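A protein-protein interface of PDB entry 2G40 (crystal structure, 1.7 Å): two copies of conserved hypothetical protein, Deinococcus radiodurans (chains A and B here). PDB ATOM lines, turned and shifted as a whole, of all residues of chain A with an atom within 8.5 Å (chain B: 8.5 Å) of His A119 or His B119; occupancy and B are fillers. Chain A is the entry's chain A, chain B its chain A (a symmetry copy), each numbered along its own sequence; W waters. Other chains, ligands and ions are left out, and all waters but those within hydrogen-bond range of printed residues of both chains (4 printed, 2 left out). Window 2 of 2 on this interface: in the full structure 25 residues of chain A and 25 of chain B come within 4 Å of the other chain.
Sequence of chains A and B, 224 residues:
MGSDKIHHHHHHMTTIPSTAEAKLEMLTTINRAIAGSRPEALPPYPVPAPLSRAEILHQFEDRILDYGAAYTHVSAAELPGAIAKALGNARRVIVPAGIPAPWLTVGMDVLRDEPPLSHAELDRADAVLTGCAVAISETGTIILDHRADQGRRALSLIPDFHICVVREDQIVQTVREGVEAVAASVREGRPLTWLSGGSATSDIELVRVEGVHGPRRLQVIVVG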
ATOM      1  N   ILE A  94      14.495  -8.672 -42.087  1.00  0.00           N
ATOM      2  CA  ILE A  94      14.522  -7.736 -40.963  1.00  0.00           C
ATOM      3  C   ILE A  94      15.903  -7.130 -40.866  1.00  0.00           C
ATOM      4  O   ILE A  94      16.881  -7.862 -40.804  1.00  0.00           O
ATOM      5  CB  ILE A  94      14.214  -8.456 -39.652  1.00  0.00           C
ATOM      6  CG1 ILE A  94      12.805  -9.016 -39.674  1.00  0.00           C
ATOM      7  CG2 ILE A  94      14.371  -7.518 -38.453  1.00  0.00           C
ATOM      8  CD1 ILE A  94      12.651 -10.240 -38.757  1.00  0.00           C
ATOM      9  N   ASP A 113      12.522  -2.540 -37.380  1.00  0.00           N
ATOM     10  CA  ASP A 113      12.041  -2.886 -36.061  1.00  0.00           C
ATOM     11  C   ASP A 113      11.694  -1.654 -35.244  1.00  0.00           C
ATOM     12  O   ASP A 113      11.724  -1.702 -34.024  1.00  0.00           O
ATOM     13  CB  ASP A 113      13.101  -3.689 -35.313  1.00  0.00           C
ATOM     14  CG  ASP A 113      12.530  -4.396 -34.121  1.00  0.00           C
ATOM     15  OD1 ASP A 113      11.392  -4.897 -34.246  1.00  0.00           O
ATOM     16  OD2 ASP A 113      13.217  -4.442 -33.072  1.00  0.00           O
ATOM     17  N   PRO A 116       8.520  -1.694 -32.860  1.00  0.00           N
ATOM     18  CA  PRO A 116       8.957  -3.070 -32.766  1.00  0.00           C
ATOM     19  C   PRO A 116       8.032  -4.016 -33.512  1.00  0.00           C
ATOM     20  O   PRO A 116       6.805  -3.875 -33.443  1.00  0.00           O
ATOM     21  CB  PRO A 116       8.941  -3.355 -31.257  1.00  0.00           C
ATOM     22  CG  PRO A 116       8.981  -2.048 -30.624  1.00  0.00           C
ATOM     23  CD  PRO A 116       8.212  -1.135 -31.535  1.00  0.00           C
ATOM     24  N   LEU A 117       8.625  -4.934 -34.265  1.00  0.00           N
ATOM     25  CA  LEU A 117       7.857  -5.918 -35.003  1.00  0.00           C
ATOM     26  C   LEU A 117       7.191  -6.887 -34.030  1.00  0.00           C
ATOM     27  O   LEU A 117       7.821  -7.352 -33.098  1.00  0.00           O
ATOM     28  CB  LEU A 117       8.778  -6.696 -35.944  1.00  0.00           C
ATOM     29  CG  LEU A 117       9.454  -5.860 -37.048  1.00  0.00           C
ATOM     30  CD1 LEU A 117      10.626  -6.565 -37.577  1.00  0.00           C
ATOM     31  CD2 LEU A 117       8.474  -5.556 -38.173  1.00  0.00           C
ATOM     32  N   SER A 118       5.933  -7.222 -34.274  1.00  0.00           N
ATOM     33  CA  SER A 118       5.255  -8.219 -33.446  1.00  0.00           C
ATOM     34  C   SER A 118       5.863  -9.606 -33.657  1.00  0.00           C
ATOM     35  O   SER A 118       6.529  -9.841 -34.659  1.00  0.00           O
ATOM     36  CB  SER A 118       3.788  -8.285 -33.835  1.00  0.00           C
ATOM     37  OG  SER A 118       3.661  -8.797 -35.147  1.00  0.00           O
ATOM     38  N   HIS A 119       5.588 -10.538 -32.745  1.00  0.00           N
ATOM     39  CA  HIS A 119       6.029 -11.932 -32.926  1.00  0.00           C
ATOM     40  C   HIS A 119       5.588 -12.464 -34.289  1.00  0.00           C
ATOM     41  O   HIS A 119       6.343 -13.141 -34.985  1.00  0.00           O
ATOM     42  CB  HIS A 119       5.447 -12.847 -31.844  1.00  0.00           C
ATOM     43  CG  HIS A 119       5.881 -12.498 -30.452  1.00  0.00           C
ATOM     44  ND1 HIS A 119       5.074 -12.684 -29.346  1.00  0.00           N
ATOM     45  CD2 HIS A 119       7.032 -11.953 -29.989  1.00  0.00           C
ATOM     46  CE1 HIS A 119       5.712 -12.275 -28.263  1.00  0.00           C
ATOM     47  NE2 HIS A 119       6.902 -11.826 -28.626  1.00  0.00           N
ATOM     48  N   ALA A 120       4.363 -12.147 -34.671  1.00  0.00           N
ATOM     49  CA  ALA A 120       3.808 -12.632 -35.936  1.00  0.00           C
ATOM     50  C   ALA A 120       4.549 -12.031 -37.128  1.00  0.00           C
ATOM     51  O   ALA A 120       4.843 -12.729 -38.085  1.00  0.00           O
ATOM     52  CB  ALA A 120       2.340 -12.315 -36.010  1.00  0.00           C
ATOM     53  N   GLU A 121       4.851 -10.735 -37.057  1.00  0.00           N
ATOM     54  CA  GLU A 121       5.658 -10.076 -38.092  1.00  0.00           C
ATOM     55  C   GLU A 121       7.044 -10.705 -38.178  1.00  0.00           C
ATOM     56  O   GLU A 121       7.577 -10.938 -39.267  1.00  0.00           O
ATOM     57  CB  GLU A 121       5.756  -8.566 -37.841  1.00  0.00           C
ATOM     58  CG  GLU A 121       4.496  -7.816 -38.308  1.00  0.00           C
ATOM     59  CD  GLU A 121       4.282  -6.444 -37.662  1.00  0.00           C
ATOM     60  OE1 GLU A 121       4.806  -6.161 -36.562  1.00  0.00           O
ATOM     61  OE2 GLU A 121       3.525  -5.639 -38.251  1.00  0.00           O
ATOM     62  N   LEU A 122       7.649 -10.964 -37.027  1.00  0.00           N
ATOM     63  CA  LEU A 122       8.958 -11.640 -37.014  1.00  0.00           C
ATOM     64  C   LEU A 122       8.884 -13.056 -37.566  1.00  0.00           C
ATOM     65  O   LEU A 122       9.781 -13.511 -38.271  1.00  0.00           O
ATOM     66  CB  LEU A 122       9.506 -11.695 -35.600  1.00  0.00           C
ATOM     67  CG  LEU A 122       9.849 -10.314 -35.065  1.00  0.00           C
ATOM     68  CD1 LEU A 122      10.162 -10.415 -33.609  1.00  0.00           C
ATOM     69  CD2 LEU A 122      11.016  -9.747 -35.855  1.00  0.00           C
ATOM     70  N   ASP A 123       7.812 -13.759 -37.224  1.00  0.00           N
ATOM     71  CA  ASP A 123       7.648 -15.132 -37.686  1.00  0.00           C
ATOM     72  C   ASP A 123       7.398 -15.177 -39.194  1.00  0.00           C
ATOM     73  O   ASP A 123       7.809 -16.126 -39.864  1.00  0.00           O
ATOM     74  CB  ASP A 123       6.516 -15.812 -36.919  1.00  0.00           C
ATOM     75  CG  ASP A 123       6.418 -17.276 -37.226  1.00  0.00           C
ATOM     76  OD1 ASP A 123       7.434 -17.976 -37.067  1.00  0.00           O
ATOM     77  OD2 ASP A 123       5.333 -17.728 -37.643  1.00  0.00           O
ATOM     78  N   ARG A 124       6.761 -14.141 -39.736  1.00  0.00           N
ATOM     79  CA  ARG A 124       6.442 -14.100 -41.163  1.00  0.00           C
ATOM     80  C   ARG A 124       7.595 -13.589 -42.041  1.00  0.00           C
ATOM     81  O   ARG A 124       7.598 -13.808 -43.250  1.00  0.00           O
ATOM     82  CB  ARG A 124       5.176 -13.277 -41.387  1.00  0.00           C
ATOM     83  CG  ARG A 124       3.912 -14.060 -40.993  1.00  0.00           C
ATOM     84  CD  ARG A 124       2.680 -13.165 -40.796  1.00  0.00           C
ATOM     85  N   ALA A 125       8.566 -12.929 -41.423  1.00  0.00           N
ATOM     86  CA  ALA A 125       9.735 -12.434 -42.123  1.00  0.00           C
ATOM     87  C   ALA A 125      10.490 -13.631 -42.692  1.00  0.00           C
ATOM     88  O   ALA A 125      10.439 -14.727 -42.126  1.00  0.00           O
ATOM     89  CB  ALA A 125      10.619 -11.636 -41.155  1.00  0.00           C
ATOM     90  N   ARG A 152      17.455  -6.172 -31.063  1.00  0.00           N
ATOM     91  CA  ARG A 152      17.048  -6.851 -29.826  1.00  0.00           C
ATOM     92  C   ARG A 152      17.040  -8.358 -29.996  1.00  0.00           C
ATOM     93  O   ARG A 152      17.064  -8.868 -31.106  1.00  0.00           O
ATOM     94  CB  ARG A 152      15.690  -6.346 -29.343  1.00  0.00           C
ATOM     95  CG  ARG A 152      14.539  -6.659 -30.284  1.00  0.00           C
ATOM     96  CD  ARG A 152      13.328  -5.809 -29.983  1.00  0.00           C
ATOM     97  NE  ARG A 152      12.372  -5.857 -31.060  1.00  0.00           N
ATOM     98  CZ  ARG A 152      11.274  -6.609 -31.075  1.00  0.00           C
ATOM     99  NH1 ARG A 152      10.881  -7.300 -30.005  1.00  0.00           N
ATOM    100  NH2 ARG A 152      10.508  -6.595 -32.141  1.00  0.00           N
ATOM    101  N   ALA A 154      14.858 -10.664 -29.783  1.00  0.00           N
ATOM    102  CA  ALA A 154      13.787 -11.311 -30.528  1.00  0.00           C
ATOM    103  C   ALA A 154      14.103 -11.438 -32.009  1.00  0.00           C
ATOM    104  O   ALA A 154      13.639 -12.367 -32.638  1.00  0.00           O
ATOM    105  CB  ALA A 154      12.473 -10.563 -30.355  1.00  0.00           C
ATOM    106  N   LEU A 155      14.860 -10.488 -32.556  1.00  0.00           N
ATOM    107  CA  LEU A 155      15.088 -10.425 -33.999  1.00  0.00           C
ATOM    108  C   LEU A 155      15.906 -11.591 -34.513  1.00  0.00           C
ATOM    109  O   LEU A 155      15.767 -11.970 -35.667  1.00  0.00           O
ATOM    110  CB  LEU A 155      15.808  -9.137 -34.375  1.00  0.00           C
ATOM    111  CG  LEU A 155      15.144  -7.805 -34.085  1.00  0.00           C
ATOM    112  CD1 LEU A 155      15.884  -6.712 -34.847  1.00  0.00           C
ATOM    113  CD2 LEU A 155      13.694  -7.833 -34.457  1.00  0.00           C
ATOM    114  N   LEU A 157      15.964 -14.524 -32.741  1.00  0.00           N
ATOM    115  CA  LEU A 157      15.390 -15.722 -32.172  1.00  0.00           C
ATOM    116  C   LEU A 157      14.189 -16.225 -32.931  1.00  0.00           C
ATOM    117  O   LEU A 157      14.034 -17.418 -33.113  1.00  0.00           O
ATOM    118  CB  LEU A 157      14.971 -15.489 -30.723  1.00  0.00           C
ATOM    119  CG  LEU A 157      14.343 -16.755 -30.113  1.00  0.00           C
ATOM    120  CD1 LEU A 157      15.407 -17.834 -29.925  1.00  0.00           C
ATOM    121  CD2 LEU A 157      13.637 -16.471 -28.831  1.00  0.00           C
ATOM    122  N   ILE A 158      13.310 -15.310 -33.317  1.00  0.00           N
ATOM    123  CA  ILE A 158      12.018 -15.675 -33.890  1.00  0.00           C
ATOM    124  C   ILE A 158      12.056 -15.975 -35.398  1.00  0.00           C
ATOM    125  O   ILE A 158      11.464 -16.963 -35.846  1.00  0.00           O
ATOM    126  CB  ILE A 158      10.953 -14.594 -33.589  1.00  0.00           C
ATOM    127  CG1 ILE A 158      10.878 -14.316 -32.076  1.00  0.00           C
ATOM    128  CG2 ILE A 158       9.592 -15.013 -34.135  1.00  0.00           C
ATOM    129  CD1 ILE A 158      10.569 -15.527 -31.238  1.00  0.00           C
ATOM    130  N   PRO A 159      12.728 -15.114 -36.205  1.00  0.00           N
ATOM    131  CA  PRO A 159      12.772 -15.479 -37.623  1.00  0.00           C
ATOM    132  C   PRO A 159      13.540 -16.788 -37.850  1.00  0.00           C
ATOM    133  O   PRO A 159      14.399 -17.146 -37.052  1.00  0.00           O
ATOM    134  CB  PRO A 159      13.527 -14.303 -38.267  1.00  0.00           C
ATOM    135  CG  PRO A 159      13.359 -13.184 -37.292  1.00  0.00           C
ATOM    136  CD  PRO A 159      13.423 -13.849 -35.964  1.00  0.00           C
ATOM    137  N   GLY A 211      12.487 -21.191 -36.012  1.00  0.00           N
ATOM    138  CA  GLY A 211      12.239 -22.487 -35.411  1.00  0.00           C
ATOM    139  C   GLY A 211      11.974 -22.425 -33.912  1.00  0.00           C
ATOM    140  O   GLY A 211      12.171 -21.390 -33.276  1.00  0.00           O
ATOM    141  N   VAL A 212      11.500 -23.550 -33.377  1.00  0.00           N
ATOM    142  CA  VAL A 212      11.219 -23.736 -31.941  1.00  0.00           C
ATOM    143  C   VAL A 212      12.408 -23.308 -31.082  1.00  0.00           C
ATOM    144  O   VAL A 212      12.236 -22.605 -30.099  1.00  0.00           O
ATOM    145  CB  VAL A 212      10.909 -25.223 -31.630  1.00  0.00           C
ATOM    146  CG1 VAL A 212      10.913 -25.522 -30.129  1.00  0.00           C
ATOM    147  CG2 VAL A 212       9.580 -25.637 -32.222  1.00  0.00           C
ATOM    148  N   ILE B  94       5.745 -20.847 -16.477  1.00  0.00           N
ATOM    149  CA  ILE B  94       6.338 -21.812 -17.403  1.00  0.00           C
ATOM    150  C   ILE B  94       7.463 -22.535 -16.700  1.00  0.00           C
ATOM    151  O   ILE B  94       8.354 -21.890 -16.165  1.00  0.00           O
ATOM    152  CB  ILE B  94       6.908 -21.104 -18.631  1.00  0.00           C
ATOM    153  CG1 ILE B  94       5.800 -20.426 -19.413  1.00  0.00           C
ATOM    154  CG2 ILE B  94       7.649 -22.084 -19.543  1.00  0.00           C
ATOM    155  CD1 ILE B  94       6.308 -19.218 -20.216  1.00  0.00           C
ATOM    156  N   ASP B 113       6.349 -26.915 -21.622  1.00  0.00           N
ATOM    157  CA  ASP B 113       6.751 -26.565 -22.966  1.00  0.00           C
ATOM    158  C   ASP B 113       6.838 -27.785 -23.866  1.00  0.00           C
ATOM    159  O   ASP B 113       7.573 -27.773 -24.842  1.00  0.00           O
ATOM    160  CB  ASP B 113       8.112 -25.875 -22.941  1.00  0.00           C
ATOM    161  CG  ASP B 113       8.398 -25.155 -24.223  1.00  0.00           C
ATOM    162  OD1 ASP B 113       7.445 -24.556 -24.767  1.00  0.00           O
ATOM    163  OD2 ASP B 113       9.566 -25.195 -24.681  1.00  0.00           O
ATOM    164  N   PRO B 116       5.646 -27.541 -27.645  1.00  0.00           N
ATOM    165  CA  PRO B 116       6.171 -26.210 -27.432  1.00  0.00           C
ATOM    166  C   PRO B 116       5.070 -25.169 -27.333  1.00  0.00           C
ATOM    167  O   PRO B 116       4.102 -25.208 -28.103  1.00  0.00           O
ATOM    168  CB  PRO B 116       7.056 -25.966 -28.663  1.00  0.00           C
ATOM    169  CG  PRO B 116       7.344 -27.288 -29.191  1.00  0.00           C
ATOM    170  CD  PRO B 116       6.115 -28.108 -28.919  1.00  0.00           C
ATOM    171  N   LEU B 117       5.193 -24.285 -26.351  1.00  0.00           N
ATOM    172  CA  LEU B 117       4.226 -23.219 -26.168  1.00  0.00           C
ATOM    173  C   LEU B 117       4.331 -22.225 -27.320  1.00  0.00           C
ATOM    174  O   LEU B 117       5.420 -21.839 -27.703  1.00  0.00           O
ATOM    175  CB  LEU B 117       4.494 -22.497 -24.846  1.00  0.00           C
ATOM    176  CG  LEU B 117       4.333 -23.357 -23.578  1.00  0.00           C
ATOM    177  CD1 LEU B 117       5.038 -22.740 -22.450  1.00  0.00           C
ATOM    178  CD2 LEU B 117       2.862 -23.546 -23.236  1.00  0.00           C
ATOM    179  N   SER B 118       3.197 -21.777 -27.840  1.00  0.00           N
ATOM    180  CA  SER B 118       3.211 -20.750 -28.880  1.00  0.00           C
ATOM    181  C   SER B 118       3.699 -19.414 -28.318  1.00  0.00           C
ATOM    182  O   SER B 118       3.680 -19.209 -27.110  1.00  0.00           O
ATOM    183  CB  SER B 118       1.802 -20.549 -29.410  1.00  0.00           C
ATOM    184  OG  SER B 118       0.983 -19.993 -28.400  1.00  0.00           O
ATOM    185  N   HIS B 119       4.083 -18.487 -29.196  1.00  0.00           N
ATOM    186  CA  HIS B 119       4.454 -17.131 -28.755  1.00  0.00           C
ATOM    187  C   HIS B 119       3.353 -16.527 -27.885  1.00  0.00           C
ATOM    188  O   HIS B 119       3.619 -15.897 -26.862  1.00  0.00           O
ATOM    189  CB  HIS B 119       4.685 -16.199 -29.950  1.00  0.00           C
ATOM    190  CG  HIS B 119       5.813 -16.621 -30.842  1.00  0.00           C
ATOM    191  ND1 HIS B 119       5.814 -16.397 -32.206  1.00  0.00           N
ATOM    192  CD2 HIS B 119       6.969 -17.274 -30.569  1.00  0.00           C
ATOM    193  CE1 HIS B 119       6.923 -16.889 -32.730  1.00  0.00           C
ATOM    194  NE2 HIS B 119       7.641 -17.427 -31.758  1.00  0.00           N
ATOM    195  N   ALA B 120       2.111 -16.728 -28.291  1.00  0.00           N
ATOM    196  CA  ALA B 120       0.969 -16.164 -27.568  1.00  0.00           C
ATOM    197  C   ALA B 120       0.830 -16.794 -26.185  1.00  0.00           C
ATOM    198  O   ALA B 120       0.574 -16.097 -25.215  1.00  0.00           O
ATOM    199  CB  ALA B 120      -0.291 -16.354 -28.365  1.00  0.00           C
ATOM    200  N   GLU B 121       1.007 -18.111 -26.102  1.00  0.00           N
ATOM    201  CA  GLU B 121       1.007 -18.809 -24.809  1.00  0.00           C
ATOM    202  C   GLU B 121       2.135 -18.297 -23.920  1.00  0.00           C
ATOM    203  O   GLU B 121       1.956 -18.080 -22.717  1.00  0.00           O
ATOM    204  CB  GLU B 121       1.104 -20.327 -24.998  1.00  0.00           C
ATOM    205  CG  GLU B 121      -0.252 -20.955 -25.367  1.00  0.00           C
ATOM    206  CD  GLU B 121      -0.168 -22.321 -26.054  1.00  0.00           C
ATOM    207  OE1 GLU B 121       0.870 -22.678 -26.655  1.00  0.00           O
ATOM    208  OE2 GLU B 121      -1.191 -23.043 -26.034  1.00  0.00           O
ATOM    209  N   LEU B 122       3.313 -18.121 -24.501  1.00  0.00           N
ATOM    210  CA  LEU B 122       4.440 -17.560 -23.736  1.00  0.00           C
ATOM    211  C   LEU B 122       4.181 -16.127 -23.291  1.00  0.00           C
ATOM    212  O   LEU B 122       4.539 -15.731 -22.185  1.00  0.00           O
ATOM    213  CB  LEU B 122       5.708 -17.589 -24.571  1.00  0.00           C
ATOM    214  CG  LEU B 122       6.178 -19.008 -24.846  1.00  0.00           C
ATOM    215  CD1 LEU B 122       7.282 -18.973 -25.849  1.00  0.00           C
ATOM    216  CD2 LEU B 122       6.620 -19.651 -23.542  1.00  0.00           C
ATOM    217  N   ASP B 123       3.569 -15.346 -24.171  1.00  0.00           N
ATOM    218  CA  ASP B 123       3.284 -13.952 -23.852  1.00  0.00           C
ATOM    219  C   ASP B 123       2.212 -13.845 -22.766  1.00  0.00           C
ATOM    220  O   ASP B 123       2.238 -12.917 -21.957  1.00  0.00           O
ATOM    221  CB  ASP B 123       2.867 -13.199 -25.115  1.00  0.00           C
ATOM    222  CG  ASP B 123       2.733 -11.724 -24.881  1.00  0.00           C
ATOM    223  OD1 ASP B 123       3.709 -11.118 -24.404  1.00  0.00           O
ATOM    224  OD2 ASP B 123       1.651 -11.171 -25.156  1.00  0.00           O
ATOM    225  N   ARG B 124       1.294 -14.809 -22.721  1.00  0.00           N
ATOM    226  CA  ARG B 124       0.207 -14.784 -21.743  1.00  0.00           C
ATOM    227  C   ARG B 124       0.590 -15.366 -20.375  1.00  0.00           C
ATOM    228  O   ARG B 124      -0.089 -15.116 -19.381  1.00  0.00           O
ATOM    229  CB  ARG B 124      -1.020 -15.490 -22.315  1.00  0.00           C
ATOM    230  CG  ARG B 124      -1.751 -14.614 -23.347  1.00  0.00           C
ATOM    231  CD  ARG B 124      -2.713 -15.407 -24.245  1.00  0.00           C
ATOM    232  N   ALA B 125       1.680 -16.123 -20.334  1.00  0.00           N
ATOM    233  CA  ALA B 125       2.181 -16.696 -19.100  1.00  0.00           C
ATOM    234  C   ALA B 125       2.565 -15.552 -18.167  1.00  0.00           C
ATOM    235  O   ALA B 125       2.945 -14.472 -18.629  1.00  0.00           O
ATOM    236  CB  ALA B 125       3.391 -17.592 -19.400  1.00  0.00           C
ATOM    237  N   ARG B 152      14.313 -23.886 -23.819  1.00  0.00           N
ATOM    238  CA  ARG B 152      14.756 -23.208 -25.045  1.00  0.00           C
ATOM    239  C   ARG B 152      14.779 -21.702 -24.869  1.00  0.00           C
ATOM    240  O   ARG B 152      14.199 -21.166 -23.938  1.00  0.00           O
ATOM    241  CB  ARG B 152      13.891 -23.609 -26.238  1.00  0.00           C
ATOM    242  CG  ARG B 152      12.439 -23.175 -26.128  1.00  0.00           C
ATOM    243  CD  ARG B 152      11.559 -23.927 -27.097  1.00  0.00           C
ATOM    244  NE  ARG B 152      10.165 -23.769 -26.771  1.00  0.00           N
ATOM    245  CZ  ARG B 152       9.330 -22.927 -27.374  1.00  0.00           C
ATOM    246  NH1 ARG B 152       9.688 -22.234 -28.454  1.00  0.00           N
ATOM    247  NH2 ARG B 152       8.090 -22.847 -26.949  1.00  0.00           N
ATOM    248  N   ALA B 154      13.327 -19.226 -26.243  1.00  0.00           N
ATOM    249  CA  ALA B 154      12.083 -18.471 -26.238  1.00  0.00           C
ATOM    250  C   ALA B 154      11.492 -18.331 -24.845  1.00  0.00           C
ATOM    251  O   ALA B 154      10.830 -17.350 -24.575  1.00  0.00           O
ATOM    252  CB  ALA B 154      11.054 -19.109 -27.160  1.00  0.00           C
ATOM    253  N   LEU B 155      11.710 -19.326 -23.986  1.00  0.00           N
ATOM    254  CA  LEU B 155      11.054 -19.369 -22.680  1.00  0.00           C
ATOM    255  C   LEU B 155      11.519 -18.263 -21.756  1.00  0.00           C
ATOM    256  O   LEU B 155      10.770 -17.843 -20.885  1.00  0.00           O
ATOM    257  CB  LEU B 155      11.312 -20.703 -21.992  1.00  0.00           C
ATOM    258  CG  LEU B 155      10.828 -21.982 -22.649  1.00  0.00           C
ATOM    259  CD1 LEU B 155      10.895 -23.113 -21.629  1.00  0.00           C
ATOM    260  CD2 LEU B 155       9.439 -21.821 -23.183  1.00  0.00           C
ATOM    261  N   LEU B 157      12.840 -15.395 -23.087  1.00  0.00           N
ATOM    262  CA  LEU B 157      12.805 -14.169 -23.851  1.00  0.00           C
ATOM    263  C   LEU B 157      11.434 -13.546 -23.914  1.00  0.00           C
ATOM    264  O   LEU B 157      11.304 -12.339 -23.824  1.00  0.00           O
ATOM    265  CB  LEU B 157      13.284 -14.404 -25.281  1.00  0.00           C
ATOM    266  CG  LEU B 157      13.234 -13.107 -26.108  1.00  0.00           C
ATOM    267  CD1 LEU B 157      14.297 -12.127 -25.616  1.00  0.00           C
ATOM    268  CD2 LEU B 157      13.379 -13.364 -27.568  1.00  0.00           C
ATOM    269  N   ILE B 158      10.419 -14.372 -24.133  1.00  0.00           N
ATOM    270  CA  ILE B 158       9.071 -13.884 -24.403  1.00  0.00           C
ATOM    271  C   ILE B 158       8.255 -13.547 -23.144  1.00  0.00           C
ATOM    272  O   ILE B 158       7.599 -12.501 -23.095  1.00  0.00           O
ATOM    273  CB  ILE B 158       8.290 -14.879 -25.294  1.00  0.00           C
ATOM    274  CG1 ILE B 158       9.081 -15.190 -26.578  1.00  0.00           C
ATOM    275  CG2 ILE B 158       6.905 -14.330 -25.625  1.00  0.00           C
ATOM    276  CD1 ILE B 158       9.417 -13.980 -27.407  1.00  0.00           C
ATOM    277  N   PRO B 159       8.260 -14.440 -22.120  1.00  0.00           N
ATOM    278  CA  PRO B 159       7.506 -14.042 -20.930  1.00  0.00           C
ATOM    279  C   PRO B 159       8.109 -12.797 -20.264  1.00  0.00           C
ATOM    280  O   PRO B 159       9.298 -12.535 -20.409  1.00  0.00           O
ATOM    281  CB  PRO B 159       7.647 -15.260 -19.999  1.00  0.00           C
ATOM    282  CG  PRO B 159       7.980 -16.386 -20.922  1.00  0.00           C
ATOM    283  CD  PRO B 159       8.856 -15.765 -21.949  1.00  0.00           C
ATOM    284  N   GLY B 211       8.690  -8.372 -22.253  1.00  0.00           N
ATOM    285  CA  GLY B 211       8.947  -7.076 -22.851  1.00  0.00           C
ATOM    286  C   GLY B 211       9.594  -7.156 -24.228  1.00  0.00           C
ATOM    287  O   GLY B 211      10.034  -8.221 -24.661  1.00  0.00           O
ATOM    288  N   VAL B 212       9.614  -6.010 -24.908  1.00  0.00           N
ATOM    289  CA  VAL B 212      10.233  -5.839 -26.236  1.00  0.00           C
ATOM    290  C   VAL B 212      11.658  -6.389 -26.260  1.00  0.00           C
ATOM    291  O   VAL B 212      12.027  -7.102 -27.180  1.00  0.00           O
ATOM    292  CB  VAL B 212      10.287  -4.340 -26.629  1.00  0.00           C
ATOM    293  CG1 VAL B 212      11.184  -4.083 -27.842  1.00  0.00           C
ATOM    294  CG2 VAL B 212       8.902  -3.800 -26.905  1.00  0.00           C
HETATM  295  O   HOH W   1      13.629 -20.754 -28.701  1.00  0.00           O
HETATM  296  O   HOH W   2       9.097 -10.423 -26.550  1.00  0.00           O
HETATM  297  O   HOH W   3      10.504 -19.066 -32.219  1.00  0.00           O
HETATM  298  O   HOH W   4      13.810  -9.102 -27.564  1.00  0.00           O
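OD2 of Asp A113 is in salt-bridge range of NE of Arg A152 (2.6 Å).
The backbone carbonyl oxygen of Leu A117 is in hydrogen-bond range of the guanidinium group of Arg A152, 3.0 Å away.
The side-chain carboxylate of Asp B113 lies within salt-bridge range of the guanidinium group of Arg B152, 2.6 Å away.
The guanidinium group (NH2) of Arg B152 lies within hydrogen-bond range of the backbone carbonyl oxygen (O) of Leu B117, 3.0 Å away.
His A119 touches its own counterpart, His B119.
Arg A152 touches Val B212, and with the chains exchanged Val A212 touches Arg B152.
Ala A154 touches Leu B157, and with the chains exchanged Leu A157 touches Ala B154.
Leu A157 touches its own counterpart, Leu B157.
Of the 8 pairs that touch across the chains among the printed residues, 8 have their exchanged pair printed and touching as well.
Printed residues of chain B that touch a printed residue of chain A: His B119, Arg B152, Ala B154, Leu B157, Ile B158 and Val B212.
Hydrophobic or aromatic side chains of chain B that line the printed part of chain A: His B119, Leu B157, Ile B158 and Val B212.
Of the 20 printed residues of chain A, 6 touch a printed residue of chain B.
Hydrophobic or aromatic side chains of chain A that line the printed part of chain B: His A119, Leu A157, Ile A158 and Val A212.
The guanidinium group (NH1) of Arg A152 lies within hydrogen-bond range of the backbone carbonyl oxygen (O) of Val B212 (3.1 Å).
O of Val A212 sits at hydrogen-bond distance from NH1 of Arg B152 (3.1 Å).
Printed residues of chain A within 4 Å of His B119: His A119 and Ile A158.
No residue of chain B comes within 4 Å of Ser A118.
No residue of chain B comes within 4 Å of Ala A120.
No residue of chain A comes within 4 Å of Ser B118.
No residue of chain A comes within 4 Å of Ala B120.
Of the printed residues of chain B, Ala A154 touches Leu B157 (3.6 Å).
Of the printed residues of chain B, Ile A158 touches His B119 (3.5 Å).
Printed residues of chain A within 4 Å of Val B212: Arg A152 (3.1 Å).
Printed residues of chain A within 4 Å of Leu B157: Ala A154 and Leu A157.
Of the printed residues of chain A, Ala B154 touches Leu A157 (3.6 Å).
Ile B94 touches none of the printed residues of chain A.
The nearest printed residue of chain B that does not touch His A119 is Asp B123 (4.3 Å).
The nearest printed residue of chain A that does not touch His B119 is Asp A123 (4.3 Å).
The nearest printed residue of chain B that does not touch Arg A152 is Gly B211 (5.5 Å).
Water W1 bridges the backbone carbonyl oxygen of Val A212 (2.7 Å) and the backbone NH of Ala B154 (2.9 Å).
Water W4 bridges O of Val B212 (2.7 Å) and N of Ala A154 (2.9 Å).
Water W2 lies within hydrogen-bond range of O of Gly B211 (3.0 Å) and NE2 of His A119 (3.3 Å).
Water W3 bridges the backbone carbonyl oxygen (O) of Gly A211 and a ring nitrogen (NE2) of His B119.
His A119 touches His B119 (CB to ND1, 3.6 Å).
NE2 of His A119 touches CD1 of Ile B158 (3.5 Å).
Ala A154 touches Leu B157.
Leu A157 touches Ala B154.
Leu A157 touches Leu B157 (CD2 to CD2, 3.4 Å).
CD1 of Ile A158 touches NE2 of His B119 (3.5 Å).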
